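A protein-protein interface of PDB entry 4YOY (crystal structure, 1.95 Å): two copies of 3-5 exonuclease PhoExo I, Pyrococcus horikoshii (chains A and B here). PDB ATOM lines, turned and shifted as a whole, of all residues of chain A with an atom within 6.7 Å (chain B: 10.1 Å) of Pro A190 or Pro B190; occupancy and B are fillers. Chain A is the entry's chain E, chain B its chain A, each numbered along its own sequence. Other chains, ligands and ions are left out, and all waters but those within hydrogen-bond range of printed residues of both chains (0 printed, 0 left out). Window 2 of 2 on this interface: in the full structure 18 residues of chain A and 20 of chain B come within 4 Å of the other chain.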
ATOM      1  N   TYR A 173      21.825  32.384  -3.743  1.00  0.00           N
ATOM      2  CA  TYR A 173      21.913  32.847  -2.341  1.00  0.00           C
ATOM      3  C   TYR A 173      22.821  34.054  -2.150  1.00  0.00           C
ATOM      4  O   TYR A 173      23.858  34.012  -1.480  1.00  0.00           O
ATOM      5  CB  TYR A 173      22.270  31.705  -1.369  1.00  0.00           C
ATOM      6  CG  TYR A 173      23.327  30.711  -1.774  1.00  0.00           C
ATOM      7  CD1 TYR A 173      24.671  30.942  -1.502  1.00  0.00           C
ATOM      8  CD2 TYR A 173      22.970  29.512  -2.390  1.00  0.00           C
ATOM      9  CE1 TYR A 173      25.636  30.021  -1.865  1.00  0.00           C
ATOM     10  CE2 TYR A 173      23.926  28.578  -2.748  1.00  0.00           C
ATOM     11  CZ  TYR A 173      25.256  28.838  -2.481  1.00  0.00           C
ATOM     12  OH  TYR A 173      26.211  27.911  -2.845  1.00  0.00           O
ATOM     13  N   SER A 187      27.013  37.461  -0.141  1.00  0.00           N
ATOM     14  CA  SER A 187      26.601  36.062  -0.078  1.00  0.00           C
ATOM     15  C   SER A 187      25.694  35.868   1.136  1.00  0.00           C
ATOM     16  O   SER A 187      25.909  36.469   2.180  1.00  0.00           O
ATOM     17  CB  SER A 187      27.810  35.137  -0.007  1.00  0.00           C
ATOM     18  OG  SER A 187      27.399  33.774   0.044  1.00  0.00           O
ATOM     19  N   LEU A 188      24.647  35.067   0.979  1.00  0.00           N
ATOM     20  CA  LEU A 188      23.790  34.712   2.109  1.00  0.00           C
ATOM     21  C   LEU A 188      24.325  33.468   2.823  1.00  0.00           C
ATOM     22  O   LEU A 188      23.742  33.023   3.807  1.00  0.00           O
ATOM     23  CB  LEU A 188      22.347  34.468   1.652  1.00  0.00           C
ATOM     24  CG  LEU A 188      21.543  35.698   1.209  1.00  0.00           C
ATOM     25  CD1 LEU A 188      20.215  35.283   0.561  1.00  0.00           C
ATOM     26  CD2 LEU A 188      21.290  36.623   2.392  1.00  0.00           C
ATOM     27  N   ASP A 189      25.401  32.886   2.295  1.00  0.00           N
ATOM     28  CA  ASP A 189      25.973  31.662   2.879  1.00  0.00           C
ATOM     29  C   ASP A 189      27.146  31.997   3.794  1.00  0.00           C
ATOM     30  O   ASP A 189      28.247  32.250   3.326  1.00  0.00           O
ATOM     31  CB  ASP A 189      26.425  30.702   1.771  1.00  0.00           C
ATOM     32  CG  ASP A 189      26.791  29.299   2.299  1.00  0.00           C
ATOM     33  OD1 ASP A 189      26.766  29.094   3.529  1.00  0.00           O
ATOM     34  OD2 ASP A 189      27.109  28.414   1.462  1.00  0.00           O
ATOM     35  N   PRO A 190      26.926  31.942   5.115  1.00  0.00           N
ATOM     36  CA  PRO A 190      28.013  32.269   6.045  1.00  0.00           C
ATOM     37  C   PRO A 190      29.181  31.279   5.943  1.00  0.00           C
ATOM     38  O   PRO A 190      30.294  31.595   6.361  1.00  0.00           O
ATOM     39  CB  PRO A 190      27.335  32.203   7.410  1.00  0.00           C
ATOM     40  CG  PRO A 190      26.176  31.311   7.220  1.00  0.00           C
ATOM     41  CD  PRO A 190      25.706  31.490   5.807  1.00  0.00           C
ATOM     42  N   ARG A 191      28.937  30.110   5.357  1.00  0.00           N
ATOM     43  CA  ARG A 191      30.001  29.135   5.136  1.00  0.00           C
ATOM     44  C   ARG A 191      31.067  29.646   4.182  1.00  0.00           C
ATOM     45  O   ARG A 191      32.204  29.164   4.207  1.00  0.00           O
ATOM     46  CB  ARG A 191      29.431  27.819   4.597  1.00  0.00           C
ATOM     47  CG  ARG A 191      28.502  27.099   5.565  1.00  0.00           C
ATOM     48  CD  ARG A 191      27.932  25.852   4.910  1.00  0.00           C
ATOM     49  NE  ARG A 191      27.338  26.161   3.607  1.00  0.00           N
ATOM     50  CZ  ARG A 191      27.121  25.251   2.664  1.00  0.00           C
ATOM     51  NH1 ARG A 191      27.485  23.989   2.869  1.00  0.00           N
ATOM     52  NH2 ARG A 191      26.593  25.607   1.504  1.00  0.00           N
ATOM     53  N   GLU A 192      30.717  30.621   3.341  1.00  0.00           N
ATOM     54  CA  GLU A 192      31.685  31.148   2.382  1.00  0.00           C
ATOM     55  C   GLU A 192      32.641  32.172   2.986  1.00  0.00           C
ATOM     56  O   GLU A 192      33.637  32.533   2.361  1.00  0.00           O
ATOM     57  CB  GLU A 192      30.949  31.747   1.176  1.00  0.00           C
ATOM     58  CG  GLU A 192      30.252  30.686   0.355  1.00  0.00           C
ATOM     59  CD  GLU A 192      29.590  31.231  -0.916  1.00  0.00           C
ATOM     60  OE1 GLU A 192      29.476  30.456  -1.888  1.00  0.00           O
ATOM     61  OE2 GLU A 192      29.196  32.421  -0.939  1.00  0.00           O
ATOM     62  N   GLY A 193      32.370  32.608   4.212  1.00  0.00           N
ATOM     63  CA  GLY A 193      33.339  33.391   4.953  1.00  0.00           C
ATOM     64  C   GLY A 193      33.207  34.896   4.763  1.00  0.00           C
ATOM     65  O   GLY A 193      34.128  35.616   5.054  1.00  0.00           O
ATOM     66  N   GLY A 194      32.072  35.367   4.259  1.00  0.00           N
ATOM     67  CA  GLY A 194      31.830  36.807   4.193  1.00  0.00           C
ATOM     68  C   GLY A 194      32.210  37.465   2.880  1.00  0.00           C
ATOM     69  O   GLY A 194      32.913  38.484   2.850  1.00  0.00           O
ATOM     70  N   MET A 221      17.160  34.519  -4.857  1.00  0.00           N
ATOM     71  CA  MET A 221      16.318  35.676  -4.550  1.00  0.00           C
ATOM     72  C   MET A 221      15.910  36.407  -5.837  1.00  0.00           C
ATOM     73  O   MET A 221      16.595  36.317  -6.860  1.00  0.00           O
ATOM     74  CB  MET A 221      17.037  36.656  -3.606  1.00  0.00           C
ATOM     75  CG  MET A 221      17.533  36.018  -2.289  1.00  0.00           C
ATOM     76  SD  MET A 221      16.180  35.311  -1.306  1.00  0.00           S
ATOM     77  CE  MET A 221      16.669  33.584  -1.172  1.00  0.00           C
ATOM     78  N   LYS B  35       7.648  34.079   1.988  1.00  0.00           N
ATOM     79  CA  LYS B  35       8.480  33.765   3.152  1.00  0.00           C
ATOM     80  C   LYS B  35       7.705  33.001   4.218  1.00  0.00           C
ATOM     81  O   LYS B  35       8.307  32.291   5.005  1.00  0.00           O
ATOM     82  CB  LYS B  35       9.079  35.040   3.774  1.00  0.00           C
ATOM     83  CG  LYS B  35      10.119  35.740   2.909  1.00  0.00           C
ATOM     84  CD  LYS B  35      10.512  37.108   3.513  1.00  0.00           C
ATOM     85  CE  LYS B  35      11.619  37.775   2.710  1.00  0.00           C
ATOM     86  NZ  LYS B  35      12.077  39.061   3.303  1.00  0.00           N
ATOM     87  N   ARG B 142       8.917  24.085   1.054  1.00  0.00           N
ATOM     88  CA  ARG B 142       9.770  24.268   2.243  1.00  0.00           C
ATOM     89  C   ARG B 142       8.995  24.975   3.375  1.00  0.00           C
ATOM     90  O   ARG B 142       9.159  24.640   4.555  1.00  0.00           O
ATOM     91  CB  ARG B 142      11.027  25.059   1.882  1.00  0.00           C
ATOM     92  CG  ARG B 142      11.917  25.433   3.101  1.00  0.00           C
ATOM     93  CD  ARG B 142      12.404  24.219   3.866  1.00  0.00           C
ATOM     94  NE  ARG B 142      13.408  24.636   4.871  1.00  0.00           N
ATOM     95  CZ  ARG B 142      13.849  23.893   5.890  1.00  0.00           C
ATOM     96  NH1 ARG B 142      13.385  22.653   6.119  1.00  0.00           N
ATOM     97  NH2 ARG B 142      14.753  24.413   6.718  1.00  0.00           N
ATOM     98  N   ILE B 146       8.265  23.534   7.102  1.00  0.00           N
ATOM     99  CA  ILE B 146       8.492  24.272   8.349  1.00  0.00           C
ATOM    100  C   ILE B 146       7.235  24.234   9.217  1.00  0.00           C
ATOM    101  O   ILE B 146       7.316  24.023  10.428  1.00  0.00           O
ATOM    102  CB  ILE B 146       8.911  25.735   8.075  1.00  0.00           C
ATOM    103  CG1 ILE B 146      10.299  25.760   7.424  1.00  0.00           C
ATOM    104  CG2 ILE B 146       8.930  26.548   9.380  1.00  0.00           C
ATOM    105  CD1 ILE B 146      10.691  27.133   6.876  1.00  0.00           C
ATOM    106  N   TYR B 173      17.102  21.206   9.225  1.00  0.00           N
ATOM    107  CA  TYR B 173      17.621  22.529   9.619  1.00  0.00           C
ATOM    108  C   TYR B 173      16.559  23.590   9.836  1.00  0.00           C
ATOM    109  O   TYR B 173      16.463  24.598   9.129  1.00  0.00           O
ATOM    110  CB  TYR B 173      18.719  23.030   8.655  1.00  0.00           C
ATOM    111  CG  TYR B 173      18.552  22.841   7.162  1.00  0.00           C
ATOM    112  CD1 TYR B 173      17.876  23.786   6.393  1.00  0.00           C
ATOM    113  CD2 TYR B 173      19.151  21.760   6.508  1.00  0.00           C
ATOM    114  CE1 TYR B 173      17.745  23.639   5.006  1.00  0.00           C
ATOM    115  CE2 TYR B 173      19.019  21.602   5.113  1.00  0.00           C
ATOM    116  CZ  TYR B 173      18.322  22.551   4.381  1.00  0.00           C
ATOM    117  OH  TYR B 173      18.192  22.412   3.020  1.00  0.00           O
ATOM    118  N   MET B 174      15.725  23.326  10.830  1.00  0.00           N
ATOM    119  CA  MET B 174      14.788  24.326  11.296  1.00  0.00           C
ATOM    120  C   MET B 174      14.788  24.286  12.818  1.00  0.00           C
ATOM    121  O   MET B 174      15.140  23.277  13.423  1.00  0.00           O
ATOM    122  CB  MET B 174      13.380  24.082  10.728  1.00  0.00           C
ATOM    123  CG  MET B 174      12.738  22.762  11.188  1.00  0.00           C
ATOM    124  SD  MET B 174      10.954  22.800  10.910  1.00  0.00           S
ATOM    125  CE  MET B 174      10.367  23.931  12.180  1.00  0.00           C
ATOM    126  N   GLU B 175      14.412  25.410  13.412  1.00  0.00           N
ATOM    127  CA  GLU B 175      14.298  25.572  14.845  1.00  0.00           C
ATOM    128  C   GLU B 175      12.870  25.946  15.166  1.00  0.00           C
ATOM    129  O   GLU B 175      12.134  26.419  14.285  1.00  0.00           O
ATOM    130  CB  GLU B 175      15.243  26.662  15.352  1.00  0.00           C
ATOM    131  CG  GLU B 175      15.006  28.019  14.638  1.00  0.00           C
ATOM    132  CD  GLU B 175      15.816  29.177  15.246  1.00  0.00           C
ATOM    133  OE1 GLU B 175      16.291  29.039  16.388  1.00  0.00           O
ATOM    134  OE2 GLU B 175      16.000  30.215  14.566  1.00  0.00           O
ATOM    135  N   LYS B 186      11.375  28.547  12.213  1.00  0.00           N
ATOM    136  CA  LYS B 186      12.238  29.240  11.265  1.00  0.00           C
ATOM    137  C   LYS B 186      13.218  28.277  10.637  1.00  0.00           C
ATOM    138  O   LYS B 186      13.776  27.424  11.327  1.00  0.00           O
ATOM    139  CB  LYS B 186      13.060  30.354  11.949  1.00  0.00           C
ATOM    140  CG  LYS B 186      12.305  31.563  12.370  1.00  0.00           C
ATOM    141  CD  LYS B 186      13.095  32.285  13.476  1.00  0.00           C
ATOM    142  CE  LYS B 186      12.674  33.727  13.586  1.00  0.00           C
ATOM    143  NZ  LYS B 186      12.933  34.290  14.936  1.00  0.00           N
ATOM    144  N   SER B 187      13.494  28.470   9.355  1.00  0.00           N
ATOM    145  CA  SER B 187      14.609  27.782   8.720  1.00  0.00           C
ATOM    146  C   SER B 187      15.922  28.234   9.355  1.00  0.00           C
ATOM    147  O   SER B 187      16.079  29.412   9.694  1.00  0.00           O
ATOM    148  CB  SER B 187      14.649  28.078   7.222  1.00  0.00           C
ATOM    149  OG  SER B 187      15.731  27.398   6.618  1.00  0.00           O
ATOM    150  N   LEU B 188      16.856  27.307   9.523  1.00  0.00           N
ATOM    151  CA  LEU B 188      18.199  27.656   9.982  1.00  0.00           C
ATOM    152  C   LEU B 188      19.129  27.987   8.827  1.00  0.00           C
ATOM    153  O   LEU B 188      20.275  28.336   9.044  1.00  0.00           O
ATOM    154  CB  LEU B 188      18.803  26.520  10.821  1.00  0.00           C
ATOM    155  CG  LEU B 188      18.223  26.330  12.208  1.00  0.00           C
ATOM    156  CD1 LEU B 188      18.762  25.015  12.755  1.00  0.00           C
ATOM    157  CD2 LEU B 188      18.626  27.491  13.144  1.00  0.00           C
ATOM    158  N   ASP B 189      18.646  27.858   7.596  1.00  0.00           N
ATOM    159  CA  ASP B 189      19.480  28.146   6.435  1.00  0.00           C
ATOM    160  C   ASP B 189      19.215  29.579   5.931  1.00  0.00           C
ATOM    161  O   ASP B 189      18.169  29.837   5.323  1.00  0.00           O
ATOM    162  CB  ASP B 189      19.205  27.141   5.301  1.00  0.00           C
ATOM    163  CG  ASP B 189      20.244  27.211   4.194  1.00  0.00           C
ATOM    164  OD1 ASP B 189      21.142  28.083   4.278  1.00  0.00           O
ATOM    165  OD2 ASP B 189      20.175  26.386   3.249  1.00  0.00           O
ATOM    166  N   PRO B 190      20.149  30.509   6.179  1.00  0.00           N
ATOM    167  CA  PRO B 190      19.937  31.888   5.700  1.00  0.00           C
ATOM    168  C   PRO B 190      19.910  31.997   4.171  1.00  0.00           C
ATOM    169  O   PRO B 190      19.434  33.009   3.620  1.00  0.00           O
ATOM    170  CB  PRO B 190      21.135  32.645   6.266  1.00  0.00           C
ATOM    171  CG  PRO B 190      22.175  31.607   6.479  1.00  0.00           C
ATOM    172  CD  PRO B 190      21.465  30.336   6.815  1.00  0.00           C
ATOM    173  N   ARG B 191      20.429  30.978   3.492  1.00  0.00           N
ATOM    174  CA  ARG B 191      20.384  30.951   2.032  1.00  0.00           C
ATOM    175  C   ARG B 191      18.957  30.915   1.510  1.00  0.00           C
ATOM    176  O   ARG B 191      18.709  31.303   0.371  1.00  0.00           O
ATOM    177  CB  ARG B 191      21.163  29.749   1.488  1.00  0.00           C
ATOM    178  CG  ARG B 191      22.666  29.809   1.808  1.00  0.00           C
ATOM    179  CD  ARG B 191      23.382  28.577   1.296  1.00  0.00           C
ATOM    180  NE  ARG B 191      22.675  27.378   1.752  1.00  0.00           N
ATOM    181  CZ  ARG B 191      22.800  26.180   1.196  1.00  0.00           C
ATOM    182  NH1 ARG B 191      23.624  26.005   0.171  1.00  0.00           N
ATOM    183  NH2 ARG B 191      22.098  25.162   1.666  1.00  0.00           N
ATOM    184  N   GLU B 192      18.013  30.459   2.330  1.00  0.00           N
ATOM    185  CA  GLU B 192      16.622  30.352   1.874  1.00  0.00           C
ATOM    186  C   GLU B 192      15.879  31.693   1.955  1.00  0.00           C
ATOM    187  O   GLU B 192      14.734  31.802   1.514  1.00  0.00           O
ATOM    188  CB  GLU B 192      15.874  29.274   2.671  1.00  0.00           C
ATOM    189  CG  GLU B 192      16.451  27.874   2.438  1.00  0.00           C
ATOM    190  CD  GLU B 192      15.661  26.737   3.107  1.00  0.00           C
ATOM    191  OE1 GLU B 192      15.757  25.599   2.579  1.00  0.00           O
ATOM    192  OE2 GLU B 192      14.975  26.963   4.147  1.00  0.00           O
ATOM    193  N   GLY B 193      16.511  32.702   2.549  1.00  0.00           N
ATOM    194  CA  GLY B 193      16.007  34.068   2.457  1.00  0.00           C
ATOM    195  C   GLY B 193      15.034  34.452   3.557  1.00  0.00           C
ATOM    196  O   GLY B 193      14.325  35.459   3.449  1.00  0.00           O
ATOM    197  N   GLY B 194      15.001  33.651   4.620  1.00  0.00           N
ATOM    198  CA  GLY B 194      14.228  33.967   5.818  1.00  0.00           C
ATOM    199  C   GLY B 194      12.835  33.364   5.878  1.00  0.00           C
ATOM    200  O   GLY B 194      11.844  34.066   6.088  1.00  0.00           O
ATOM    201  N   LEU B 195      12.753  32.054   5.673  1.00  0.00           N
ATOM    202  CA  LEU B 195      11.480  31.360   5.692  1.00  0.00           C
ATOM    203  C   LEU B 195      11.054  31.049   7.124  1.00  0.00           C
ATOM    204  O   LEU B 195      11.883  30.653   7.959  1.00  0.00           O
ATOM    205  CB  LEU B 195      11.576  30.072   4.869  1.00  0.00           C
ATOM    206  CG  LEU B 195      12.124  30.262   3.447  1.00  0.00           C
ATOM    207  CD1 LEU B 195      12.163  28.928   2.700  1.00  0.00           C
ATOM    208  CD2 LEU B 195      11.308  31.299   2.647  1.00  0.00           C
ATOM    209  N   ARG B 219      22.500  18.269  10.774  1.00  0.00           N
ATOM    210  CA  ARG B 219      21.622  19.346  10.270  1.00  0.00           C
ATOM    211  C   ARG B 219      20.136  19.112  10.538  1.00  0.00           C
ATOM    212  O   ARG B 219      19.302  19.866  10.066  1.00  0.00           O
ATOM    213  CB  ARG B 219      21.843  19.594   8.771  1.00  0.00           C
ATOM    214  CG  ARG B 219      23.200  20.173   8.469  1.00  0.00           C
ATOM    215  CD  ARG B 219      23.365  20.555   7.010  1.00  0.00           C
ATOM    216  NE  ARG B 219      23.265  19.371   6.182  1.00  0.00           N
ATOM    217  CZ  ARG B 219      24.283  18.554   5.928  1.00  0.00           C
ATOM    218  NH1 ARG B 219      25.484  18.802   6.442  1.00  0.00           N
ATOM    219  NH2 ARG B 219      24.096  17.481   5.168  1.00  0.00           N
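The guanidinium group (NH1) of Arg B191 sits close to the guanidinium group (NH2) of Arg A191, 3.3 Å away.
The guanidinium group (NE) of Arg B142 is in salt-bridge range of the side-chain carboxylate (OE2) of Glu B192, at 2.9 Å. OG of Ser B187 is in hydrogen-bond range of OE2 of Glu B192 (2.6 Å). The guanidinium group (NH2) of Arg B191 lies within salt-bridge range of the side-chain carboxylate (OD2) of Asp B189, 2.8 Å away. N of Leu A188 sits at hydrogen-bond distance from O of Tyr A173. The side-chain hydroxyl (OG) of Ser A187 sits at hydrogen-bond distance from the backbone NH (N) of Asp A189 (3.1 Å). The guanidinium group of Arg A191 lies within salt-bridge range of the side-chain carboxylate of Asp A189, 2.9 Å away.
Among the printed residues, pairs that only touch across the chains: Tyr A173 with Arg B191, Leu A188 with Pro B190, Leu A188 with Arg B191, Asp A189 with Arg B191, Pro A190 with Pro B190, Met A221 with Arg B191, Met A221 with Glu B192 and Met A221 with Gly B193.
Printed residues of chain B within 4 Å of Pro A190: Pro B190 (3.6 Å). Pro B190 touches two residues of chain A. Of chain B, only Pro B190 (3.4 Å) and Arg B191 (3.9 Å) come within 4 Å of Leu A188. Of chain B, only Arg B191 (3.6 Å) comes within 4 Å of Asp A189. Gly A193 touches none of the printed residues of chain B. Printed residues of chain B within 4 Å of Arg A191: Arg B191 (3.3 Å). Printed residues of chain A within 4 Å of Gly B193: Met A221 (3.7 Å). Leu B195 touches none of the printed residues of chain A. The nearest residue of chain B that does not touch Pro A190 is Arg B191 (5.3 Å).
Of the 17 printed residues of chain B, 4 touch a printed residue of chain A. Of the 10 printed residues of chain A, 6 touch a printed residue of chain B. Among the printed residues, 9 pairs touch across the chains. Among the printed residues, no Asp or Glu carboxylate lies within 4 Å of a Lys or Arg side-chain nitrogen of the other chain.
Leu A188 touches Pro B190, but with the chains exchanged Pro A190 does not touch Leu B188 (6.9 Å). Leu A188 touches Arg B191, but with the chains exchanged Arg A191 does not touch Leu B188 (9.0 Å). Asp A189 touches Arg B191, but with the chains exchanged Arg A191 does not touch Asp B189 (6.5 Å). Pro A190 touches its own counterpart, Pro B190. 9 positions are printed for both chains.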
